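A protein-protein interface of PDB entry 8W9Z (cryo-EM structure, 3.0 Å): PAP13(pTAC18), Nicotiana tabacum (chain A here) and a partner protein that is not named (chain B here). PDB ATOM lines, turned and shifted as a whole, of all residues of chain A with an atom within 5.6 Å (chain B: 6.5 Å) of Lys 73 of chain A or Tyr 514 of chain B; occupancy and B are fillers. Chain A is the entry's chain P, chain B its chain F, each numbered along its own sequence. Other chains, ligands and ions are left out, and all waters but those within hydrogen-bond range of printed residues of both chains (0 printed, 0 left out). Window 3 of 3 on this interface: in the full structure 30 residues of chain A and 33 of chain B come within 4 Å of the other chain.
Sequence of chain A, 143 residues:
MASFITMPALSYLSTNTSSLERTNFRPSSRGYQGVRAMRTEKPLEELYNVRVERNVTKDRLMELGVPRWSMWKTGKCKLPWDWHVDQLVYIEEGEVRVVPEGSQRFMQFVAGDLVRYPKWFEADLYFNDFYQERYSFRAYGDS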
ATOM      1  N   MET A  71     -23.978 -11.919 -28.042  1.00  0.00           N
ATOM      2  CA  MET A  71     -24.588 -10.691 -27.558  1.00  0.00           C
ATOM      3  C   MET A  71     -24.159 -10.436 -26.120  1.00  0.00           C
ATOM      4  O   MET A  71     -23.751 -11.350 -25.398  1.00  0.00           O
ATOM      5  CB  MET A  71     -26.120 -10.759 -27.649  1.00  0.00           C
ATOM      6  CG  MET A  71     -26.818  -9.409 -27.631  1.00  0.00           C
ATOM      7  SD  MET A  71     -26.371  -8.385 -29.044  1.00  0.00           S
ATOM      8  CE  MET A  71     -27.424  -6.963 -28.774  1.00  0.00           C
ATOM      9  N   TRP A  72     -24.257  -9.173 -25.708  1.00  0.00           N
ATOM     10  CA  TRP A  72     -23.940  -8.782 -24.339  1.00  0.00           C
ATOM     11  C   TRP A  72     -24.632  -7.460 -24.049  1.00  0.00           C
ATOM     12  O   TRP A  72     -24.488  -6.503 -24.816  1.00  0.00           O
ATOM     13  CB  TRP A  72     -22.426  -8.657 -24.138  1.00  0.00           C
ATOM     14  CG  TRP A  72     -21.994  -8.703 -22.704  1.00  0.00           C
ATOM     15  CD1 TRP A  72     -21.874  -9.813 -21.922  1.00  0.00           C
ATOM     16  CD2 TRP A  72     -21.610  -7.592 -21.886  1.00  0.00           C
ATOM     17  NE1 TRP A  72     -21.445  -9.463 -20.665  1.00  0.00           N
ATOM     18  CE2 TRP A  72     -21.274  -8.105 -20.617  1.00  0.00           C
ATOM     19  CE3 TRP A  72     -21.520  -6.215 -22.101  1.00  0.00           C
ATOM     20  CZ2 TRP A  72     -20.857  -7.290 -19.570  1.00  0.00           C
ATOM     21  CZ3 TRP A  72     -21.104  -5.407 -21.060  1.00  0.00           C
ATOM     22  CH2 TRP A  72     -20.777  -5.947 -19.811  1.00  0.00           C
ATOM     23  N   LYS A  73     -25.378  -7.409 -22.948  1.00  0.00           N
ATOM     24  CA  LYS A  73     -26.181  -6.245 -22.597  1.00  0.00           C
ATOM     25  C   LYS A  73     -25.936  -5.873 -21.143  1.00  0.00           C
ATOM     26  O   LYS A  73     -25.825  -6.751 -20.281  1.00  0.00           O
ATOM     27  CB  LYS A  73     -27.671  -6.521 -22.832  1.00  0.00           C
ATOM     28  CG  LYS A  73     -28.531  -5.278 -22.958  1.00  0.00           C
ATOM     29  CD  LYS A  73     -29.956  -5.644 -23.338  1.00  0.00           C
ATOM     30  CE  LYS A  73     -30.660  -6.373 -22.208  1.00  0.00           C
ATOM     31  NZ  LYS A  73     -30.785  -5.514 -21.000  1.00  0.00           N
ATOM     32  N   THR A  74     -25.855  -4.572 -20.873  1.00  0.00           N
ATOM     33  CA  THR A  74     -25.548  -4.078 -19.538  1.00  0.00           C
ATOM     34  C   THR A  74     -25.914  -2.601 -19.463  1.00  0.00           C
ATOM     35  O   THR A  74     -25.804  -1.873 -20.451  1.00  0.00           O
ATOM     36  CB  THR A  74     -24.065  -4.285 -19.190  1.00  0.00           C
ATOM     37  OG1 THR A  74     -23.741  -5.677 -19.279  1.00  0.00           O
ATOM     38  CG2 THR A  74     -23.754  -3.802 -17.782  1.00  0.00           C
ATOM     39  N   GLY A  75     -26.354  -2.173 -18.281  1.00  0.00           N
ATOM     40  CA  GLY A  75     -26.688  -0.781 -18.052  1.00  0.00           C
ATOM     41  C   GLY A  75     -25.521   0.024 -17.519  1.00  0.00           C
ATOM     42  O   GLY A  75     -24.523   0.212 -18.219  1.00  0.00           O
ATOM     43  N   PHE A 130     -27.480   2.363 -21.339  1.00  0.00           N
ATOM     44  CA  PHE A 130     -27.748   1.114 -22.041  1.00  0.00           C
ATOM     45  C   PHE A 130     -26.620   0.790 -23.014  1.00  0.00           C
ATOM     46  O   PHE A 130     -26.145   1.663 -23.744  1.00  0.00           O
ATOM     47  CB  PHE A 130     -29.081   1.222 -22.780  1.00  0.00           C
ATOM     48  CG  PHE A 130     -29.516  -0.048 -23.443  1.00  0.00           C
ATOM     49  CD1 PHE A 130     -30.136  -1.047 -22.712  1.00  0.00           C
ATOM     50  CD2 PHE A 130     -29.321  -0.239 -24.799  1.00  0.00           C
ATOM     51  CE1 PHE A 130     -30.544  -2.214 -23.319  1.00  0.00           C
ATOM     52  CE2 PHE A 130     -29.727  -1.405 -25.412  1.00  0.00           C
ATOM     53  CZ  PHE A 130     -30.339  -2.394 -24.672  1.00  0.00           C
ATOM     54  N   TYR A 131     -26.192  -0.472 -23.022  1.00  0.00           N
ATOM     55  CA  TYR A 131     -25.037  -0.892 -23.805  1.00  0.00           C
ATOM     56  C   TYR A 131     -25.304  -2.246 -24.444  1.00  0.00           C
ATOM     57  O   TYR A 131     -25.760  -3.175 -23.771  1.00  0.00           O
ATOM     58  CB  TYR A 131     -23.782  -0.960 -22.925  1.00  0.00           C
ATOM     59  CG  TYR A 131     -22.546  -1.475 -23.631  1.00  0.00           C
ATOM     60  CD1 TYR A 131     -21.739  -0.620 -24.372  1.00  0.00           C
ATOM     61  CD2 TYR A 131     -22.178  -2.811 -23.544  1.00  0.00           C
ATOM     62  CE1 TYR A 131     -20.608  -1.086 -25.015  1.00  0.00           C
ATOM     63  CE2 TYR A 131     -21.049  -3.285 -24.184  1.00  0.00           C
ATOM     64  CZ  TYR A 131     -20.268  -2.418 -24.917  1.00  0.00           C
ATOM     65  OH  TYR A 131     -19.141  -2.886 -25.554  1.00  0.00           O
ATOM     66  N   GLN A 132     -25.014  -2.353 -25.740  1.00  0.00           N
ATOM     67  CA  GLN A 132     -25.093  -3.611 -26.466  1.00  0.00           C
ATOM     68  C   GLN A 132     -23.892  -3.720 -27.395  1.00  0.00           C
ATOM     69  O   GLN A 132     -23.379  -2.711 -27.887  1.00  0.00           O
ATOM     70  CB  GLN A 132     -26.393  -3.733 -27.271  1.00  0.00           C
ATOM     71  CG  GLN A 132     -27.622  -4.039 -26.433  1.00  0.00           C
ATOM     72  CD  GLN A 132     -28.876  -4.186 -27.273  1.00  0.00           C
ATOM     73  OE1 GLN A 132     -28.931  -3.723 -28.412  1.00  0.00           O
ATOM     74  NE2 GLN A 132     -29.889  -4.838 -26.715  1.00  0.00           N
ATOM     75  N   HIS B 403     -22.900 -11.467 -13.112  1.00  0.00           N
ATOM     76  CA  HIS B 403     -22.983 -10.265 -13.928  1.00  0.00           C
ATOM     77  C   HIS B 403     -22.987  -9.023 -13.040  1.00  0.00           C
ATOM     78  O   HIS B 403     -23.591  -9.033 -11.964  1.00  0.00           O
ATOM     79  CB  HIS B 403     -24.245 -10.288 -14.785  1.00  0.00           C
ATOM     80  CG  HIS B 403     -24.229  -9.307 -15.914  1.00  0.00           C
ATOM     81  ND1 HIS B 403     -24.581  -7.985 -15.755  1.00  0.00           N
ATOM     82  CD2 HIS B 403     -23.912  -9.457 -17.221  1.00  0.00           C
ATOM     83  CE1 HIS B 403     -24.478  -7.362 -16.915  1.00  0.00           C
ATOM     84  NE2 HIS B 403     -24.073  -8.232 -17.822  1.00  0.00           N
ATOM     85  N   TYR B 405     -24.536  -6.216 -13.396  1.00  0.00           N
ATOM     86  CA  TYR B 405     -25.863  -5.624 -13.282  1.00  0.00           C
ATOM     87  C   TYR B 405     -26.780  -6.412 -12.357  1.00  0.00           C
ATOM     88  O   TYR B 405     -27.899  -5.958 -12.092  1.00  0.00           O
ATOM     89  CB  TYR B 405     -26.498  -5.503 -14.671  1.00  0.00           C
ATOM     90  CG  TYR B 405     -27.643  -4.518 -14.757  1.00  0.00           C
ATOM     91  CD1 TYR B 405     -27.404  -3.153 -14.840  1.00  0.00           C
ATOM     92  CD2 TYR B 405     -28.960  -4.952 -14.770  1.00  0.00           C
ATOM     93  CE1 TYR B 405     -28.444  -2.249 -14.924  1.00  0.00           C
ATOM     94  CE2 TYR B 405     -30.008  -4.056 -14.853  1.00  0.00           C
ATOM     95  CZ  TYR B 405     -29.745  -2.705 -14.930  1.00  0.00           C
ATOM     96  OH  TYR B 405     -30.786  -1.809 -15.013  1.00  0.00           O
ATOM     97  N   VAL B 406     -26.334  -7.567 -11.858  1.00  0.00           N
ATOM     98  CA  VAL B 406     -27.181  -8.381 -10.990  1.00  0.00           C
ATOM     99  C   VAL B 406     -27.557  -7.610  -9.734  1.00  0.00           C
ATOM    100  O   VAL B 406     -28.730  -7.561  -9.350  1.00  0.00           O
ATOM    101  CB  VAL B 406     -26.480  -9.708 -10.649  1.00  0.00           C
ATOM    102  N   LEU B 409     -29.861  -4.538 -10.496  1.00  0.00           N
ATOM    103  CA  LEU B 409     -31.238  -4.901 -10.807  1.00  0.00           C
ATOM    104  C   LEU B 409     -31.944  -5.488  -9.591  1.00  0.00           C
ATOM    105  O   LEU B 409     -33.135  -5.236  -9.381  1.00  0.00           O
ATOM    106  CB  LEU B 409     -31.271  -5.883 -11.979  1.00  0.00           C
ATOM    107  CG  LEU B 409     -32.647  -6.270 -12.523  1.00  0.00           C
ATOM    108  CD1 LEU B 409     -33.467  -5.034 -12.843  1.00  0.00           C
ATOM    109  CD2 LEU B 409     -32.504  -7.146 -13.756  1.00  0.00           C
ATOM    110  N   ILE B 509     -36.221 -13.560 -13.776  1.00  0.00           N
ATOM    111  CA  ILE B 509     -35.947 -14.113 -15.099  1.00  0.00           C
ATOM    112  C   ILE B 509     -34.950 -13.238 -15.849  1.00  0.00           C
ATOM    113  O   ILE B 509     -34.056 -13.743 -16.537  1.00  0.00           O
ATOM    114  CB  ILE B 509     -37.259 -14.291 -15.885  1.00  0.00           C
ATOM    115  CG1 ILE B 509     -38.103 -15.408 -15.267  1.00  0.00           C
ATOM    116  CG2 ILE B 509     -36.976 -14.591 -17.350  1.00  0.00           C
ATOM    117  CD1 ILE B 509     -39.420 -15.641 -15.973  1.00  0.00           C
ATOM    118  N   GLU B 510     -35.073 -11.915 -15.716  1.00  0.00           N
ATOM    119  CA  GLU B 510     -34.126 -11.019 -16.375  1.00  0.00           C
ATOM    120  C   GLU B 510     -32.728 -11.159 -15.781  1.00  0.00           C
ATOM    121  O   GLU B 510     -31.729 -11.156 -16.514  1.00  0.00           O
ATOM    122  CB  GLU B 510     -34.613  -9.575 -16.276  1.00  0.00           C
ATOM    123  CG  GLU B 510     -33.725  -8.568 -16.987  1.00  0.00           C
ATOM    124  CD  GLU B 510     -34.277  -7.157 -16.925  1.00  0.00           C
ATOM    125  OE1 GLU B 510     -35.409  -6.982 -16.429  1.00  0.00           O
ATOM    126  OE2 GLU B 510     -33.578  -6.223 -17.372  1.00  0.00           O
ATOM    127  N   MET B 511     -32.637 -11.279 -14.454  1.00  0.00           N
ATOM    128  CA  MET B 511     -31.338 -11.506 -13.825  1.00  0.00           C
ATOM    129  C   MET B 511     -30.736 -12.832 -14.272  1.00  0.00           C
ATOM    130  O   MET B 511     -29.523 -12.931 -14.499  1.00  0.00           O
ATOM    131  CB  MET B 511     -31.472 -11.461 -12.303  1.00  0.00           C
ATOM    132  CG  MET B 511     -31.832 -10.091 -11.753  1.00  0.00           C
ATOM    133  SD  MET B 511     -31.728 -10.003  -9.953  1.00  0.00           S
ATOM    134  CE  MET B 511     -32.915 -11.258  -9.482  1.00  0.00           C
ATOM    135  N   ASP B 512     -31.571 -13.863 -14.417  1.00  0.00           N
ATOM    136  CA  ASP B 512     -31.079 -15.152 -14.890  1.00  0.00           C
ATOM    137  C   ASP B 512     -30.602 -15.063 -16.334  1.00  0.00           C
ATOM    138  O   ASP B 512     -29.607 -15.693 -16.703  1.00  0.00           O
ATOM    139  CB  ASP B 512     -32.170 -16.214 -14.747  1.00  0.00           C
ATOM    140  CG  ASP B 512     -31.638 -17.625 -14.914  1.00  0.00           C
ATOM    141  OD1 ASP B 512     -30.402 -17.797 -14.951  1.00  0.00           O
ATOM    142  OD2 ASP B 512     -32.458 -18.563 -15.007  1.00  0.00           O
ATOM    143  N   GLU B 513     -31.289 -14.274 -17.163  1.00  0.00           N
ATOM    144  CA  GLU B 513     -30.850 -14.095 -18.544  1.00  0.00           C
ATOM    145  C   GLU B 513     -29.525 -13.345 -18.611  1.00  0.00           C
ATOM    146  O   GLU B 513     -28.664 -13.661 -19.443  1.00  0.00           O
ATOM    147  CB  GLU B 513     -31.923 -13.362 -19.350  1.00  0.00           C
ATOM    148  CG  GLU B 513     -33.191 -14.171 -19.583  1.00  0.00           C
ATOM    149  CD  GLU B 513     -32.967 -15.370 -20.486  1.00  0.00           C
ATOM    150  OE1 GLU B 513     -32.002 -15.351 -21.280  1.00  0.00           O
ATOM    151  OE2 GLU B 513     -33.757 -16.333 -20.401  1.00  0.00           O
ATOM    152  N   TYR B 514     -29.343 -12.343 -17.747  1.00  0.00           N
ATOM    153  CA  TYR B 514     -28.059 -11.650 -17.679  1.00  0.00           C
ATOM    154  C   TYR B 514     -26.948 -12.601 -17.249  1.00  0.00           C
ATOM    155  O   TYR B 514     -25.855 -12.610 -17.832  1.00  0.00           O
ATOM    156  CB  TYR B 514     -28.152 -10.462 -16.723  1.00  0.00           C
ATOM    157  CG  TYR B 514     -28.933  -9.294 -17.273  1.00  0.00           C
ATOM    158  CD1 TYR B 514     -29.130  -9.146 -18.639  1.00  0.00           C
ATOM    159  CD2 TYR B 514     -29.471  -8.334 -16.428  1.00  0.00           C
ATOM    160  CE1 TYR B 514     -29.843  -8.078 -19.146  1.00  0.00           C
ATOM    161  CE2 TYR B 514     -30.185  -7.263 -16.926  1.00  0.00           C
ATOM    162  CZ  TYR B 514     -30.367  -7.140 -18.284  1.00  0.00           C
ATOM    163  OH  TYR B 514     -31.079  -6.073 -18.782  1.00  0.00           O
ATOM    164  N   ASP B 515     -27.213 -13.411 -16.220  1.00  0.00           N
ATOM    165  CA  ASP B 515     -26.236 -14.406 -15.794  1.00  0.00           C
ATOM    166  C   ASP B 515     -25.919 -15.377 -16.925  1.00  0.00           C
ATOM    167  O   ASP B 515     -24.760 -15.762 -17.118  1.00  0.00           O
ATOM    168  CB  ASP B 515     -26.757 -15.156 -14.567  1.00  0.00           C
ATOM    169  CG  ASP B 515     -25.649 -15.817 -13.767  1.00  0.00           C
ATOM    170  OD1 ASP B 515     -24.636 -16.232 -14.366  1.00  0.00           O
ATOM    171  OD2 ASP B 515     -25.796 -15.921 -12.531  1.00  0.00           O
ATOM    172  N   PHE B 516     -26.932 -15.756 -17.705  1.00  0.00           N
ATOM    173  CA  PHE B 516     -26.728 -16.711 -18.788  1.00  0.00           C
ATOM    174  C   PHE B 516     -25.878 -16.117 -19.903  1.00  0.00           C
ATOM    175  O   PHE B 516     -24.982 -16.787 -20.430  1.00  0.00           O
ATOM    176  CB  PHE B 516     -28.077 -17.181 -19.330  1.00  0.00           C
ATOM    177  CG  PHE B 516     -27.972 -18.045 -20.552  1.00  0.00           C
ATOM    178  CD1 PHE B 516     -27.576 -19.368 -20.449  1.00  0.00           C
ATOM    179  CD2 PHE B 516     -28.276 -17.537 -21.804  1.00  0.00           C
ATOM    180  CE1 PHE B 516     -27.481 -20.166 -21.573  1.00  0.00           C
ATOM    181  CE2 PHE B 516     -28.182 -18.331 -22.930  1.00  0.00           C
ATOM    182  CZ  PHE B 516     -27.784 -19.646 -22.814  1.00  0.00           C
ATOM    183  N   ILE B 517     -26.139 -14.864 -20.281  1.00  0.00           N
ATOM    184  CA  ILE B 517     -25.342 -14.266 -21.349  1.00  0.00           C
ATOM    185  C   ILE B 517     -23.912 -14.015 -20.877  1.00  0.00           C
ATOM    186  O   ILE B 517     -22.961 -14.168 -21.656  1.00  0.00           O
ATOM    187  CB  ILE B 517     -26.005 -12.983 -21.889  1.00  0.00           C
ATOM    188  CG1 ILE B 517     -26.143 -11.922 -20.800  1.00  0.00           C
ATOM    189  CG2 ILE B 517     -27.361 -13.304 -22.501  1.00  0.00           C
ATOM    190  CD1 ILE B 517     -26.836 -10.660 -21.264  1.00  0.00           C
ATOM    191  N   HIS B 518     -23.722 -13.668 -19.600  1.00  0.00           N
ATOM    192  CA  HIS B 518     -22.361 -13.517 -19.092  1.00  0.00           C
ATOM    193  C   HIS B 518     -21.633 -14.857 -19.063  1.00  0.00           C
ATOM    194  O   HIS B 518     -20.439 -14.935 -19.388  1.00  0.00           O
ATOM    195  CB  HIS B 518     -22.386 -12.884 -17.702  1.00  0.00           C
ATOM    196  CG  HIS B 518     -21.059 -12.355 -17.256  1.00  0.00           C
ATOM    197  ND1 HIS B 518     -20.069 -13.164 -16.744  1.00  0.00           N
ATOM    198  CD2 HIS B 518     -20.561 -11.096 -17.245  1.00  0.00           C
ATOM    199  CE1 HIS B 518     -19.016 -12.426 -16.437  1.00  0.00           C
ATOM    200  NE2 HIS B 518     -19.289 -11.169 -16.731  1.00  0.00           N
ATOM    201  N   TRP B 519     -22.338 -15.925 -18.680  1.00  0.00           N
ATOM    202  CA  TRP B 519     -21.740 -17.254 -18.699  1.00  0.00           C
ATOM    203  C   TRP B 519     -21.374 -17.669 -20.117  1.00  0.00           C
ATOM    204  O   TRP B 519     -20.336 -18.302 -20.337  1.00  0.00           O
ATOM    205  CB  TRP B 519     -22.696 -18.268 -18.072  1.00  0.00           C
ATOM    206  CG  TRP B 519     -22.187 -19.674 -18.116  1.00  0.00           C
ATOM    207  CD1 TRP B 519     -21.462 -20.314 -17.156  1.00  0.00           C
ATOM    208  CD2 TRP B 519     -22.365 -20.617 -19.180  1.00  0.00           C
ATOM    209  NE1 TRP B 519     -21.176 -21.596 -17.556  1.00  0.00           N
ATOM    210  CE2 TRP B 519     -21.719 -21.806 -18.794  1.00  0.00           C
ATOM    211  CE3 TRP B 519     -23.006 -20.568 -20.421  1.00  0.00           C
ATOM    212  CZ2 TRP B 519     -21.697 -22.938 -19.604  1.00  0.00           C
ATOM    213  CZ3 TRP B 519     -22.983 -21.692 -21.223  1.00  0.00           C
ATOM    214  CH2 TRP B 519     -22.333 -22.862 -20.812  1.00  0.00           C
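O of Lys 73 of chain A sits at hydrogen-bond distance from NE2 of His 403 of chain B (3.4 Å).
NE2 of His 403 of chain B sits at hydrogen-bond distance from OG1 of Thr 74 of chain A (3.0 Å).
The side-chain amino group of Lys 73 of chain A lies close to the side-chain hydroxyl of Tyr 514 of chain B, 2.3 Å away.
The backbone carbonyl oxygen of Thr 74 of chain A is in hydrogen-bond range of the backbone NH of Tyr 131 of chain A, 3.0 Å away.
The backbone NH of Tyr 405 of chain B sits at hydrogen-bond distance from a ring nitrogen (ND1) of His 403 of chain B, 2.9 Å away.
OH of Tyr 514 of chain B is in hydrogen-bond range of OE2 of Glu 510 of chain B (2.9 Å).
Among the printed residues, merely in contact across the chains: Gly 75 of chain A with Tyr 405 of chain B (3.7 Å), Trp 72 of chain A with His 403 of chain B (3.8 Å), Trp 72 of chain A with His 518 of chain B (3.9 Å) and Lys 73 of chain A with Ile 517 of chain B (3.9 Å).
Of the printed residues of chain B, Trp 72 of chain A touches His 403 (3.8 Å) and His 518 (3.9 Å).
Lys 73 of chain A touches just these residues of chain B: His 403 (3.4 Å), Tyr 514 (2.3 Å) and Ile 517 (3.9 Å).
Gln 132 of chain A touches none of the printed residues of chain B.
Printed residues of chain A within 4 Å of His 403 of chain B: Trp 72 (3.8 Å), Lys 73 (3.4 Å) and Thr 74 (3.0 Å).
Printed residues of chain A within 4 Å of Tyr 405 of chain B: Gly 75.
Of chain A, only Lys 73 comes within 4 Å of Tyr 514 of chain B.
Phe 516 of chain B touches none of the printed residues of chain A.
The nearest residue of chain B that does not touch Lys 73 of chain A is Glu 510 of chain B (4.6 Å).
Of the 15 printed residues of chain B, 5 touch a printed residue of chain A.
Along chain B the printed residues that touch a printed residue of chain A span positions 403 to 518.
Among the printed residues, 7 pairs touch across the chains.
Among the printed residues, no Asp or Glu carboxylate lies within 4 Å of a Lys or Arg side-chain nitrogen of the other chain.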
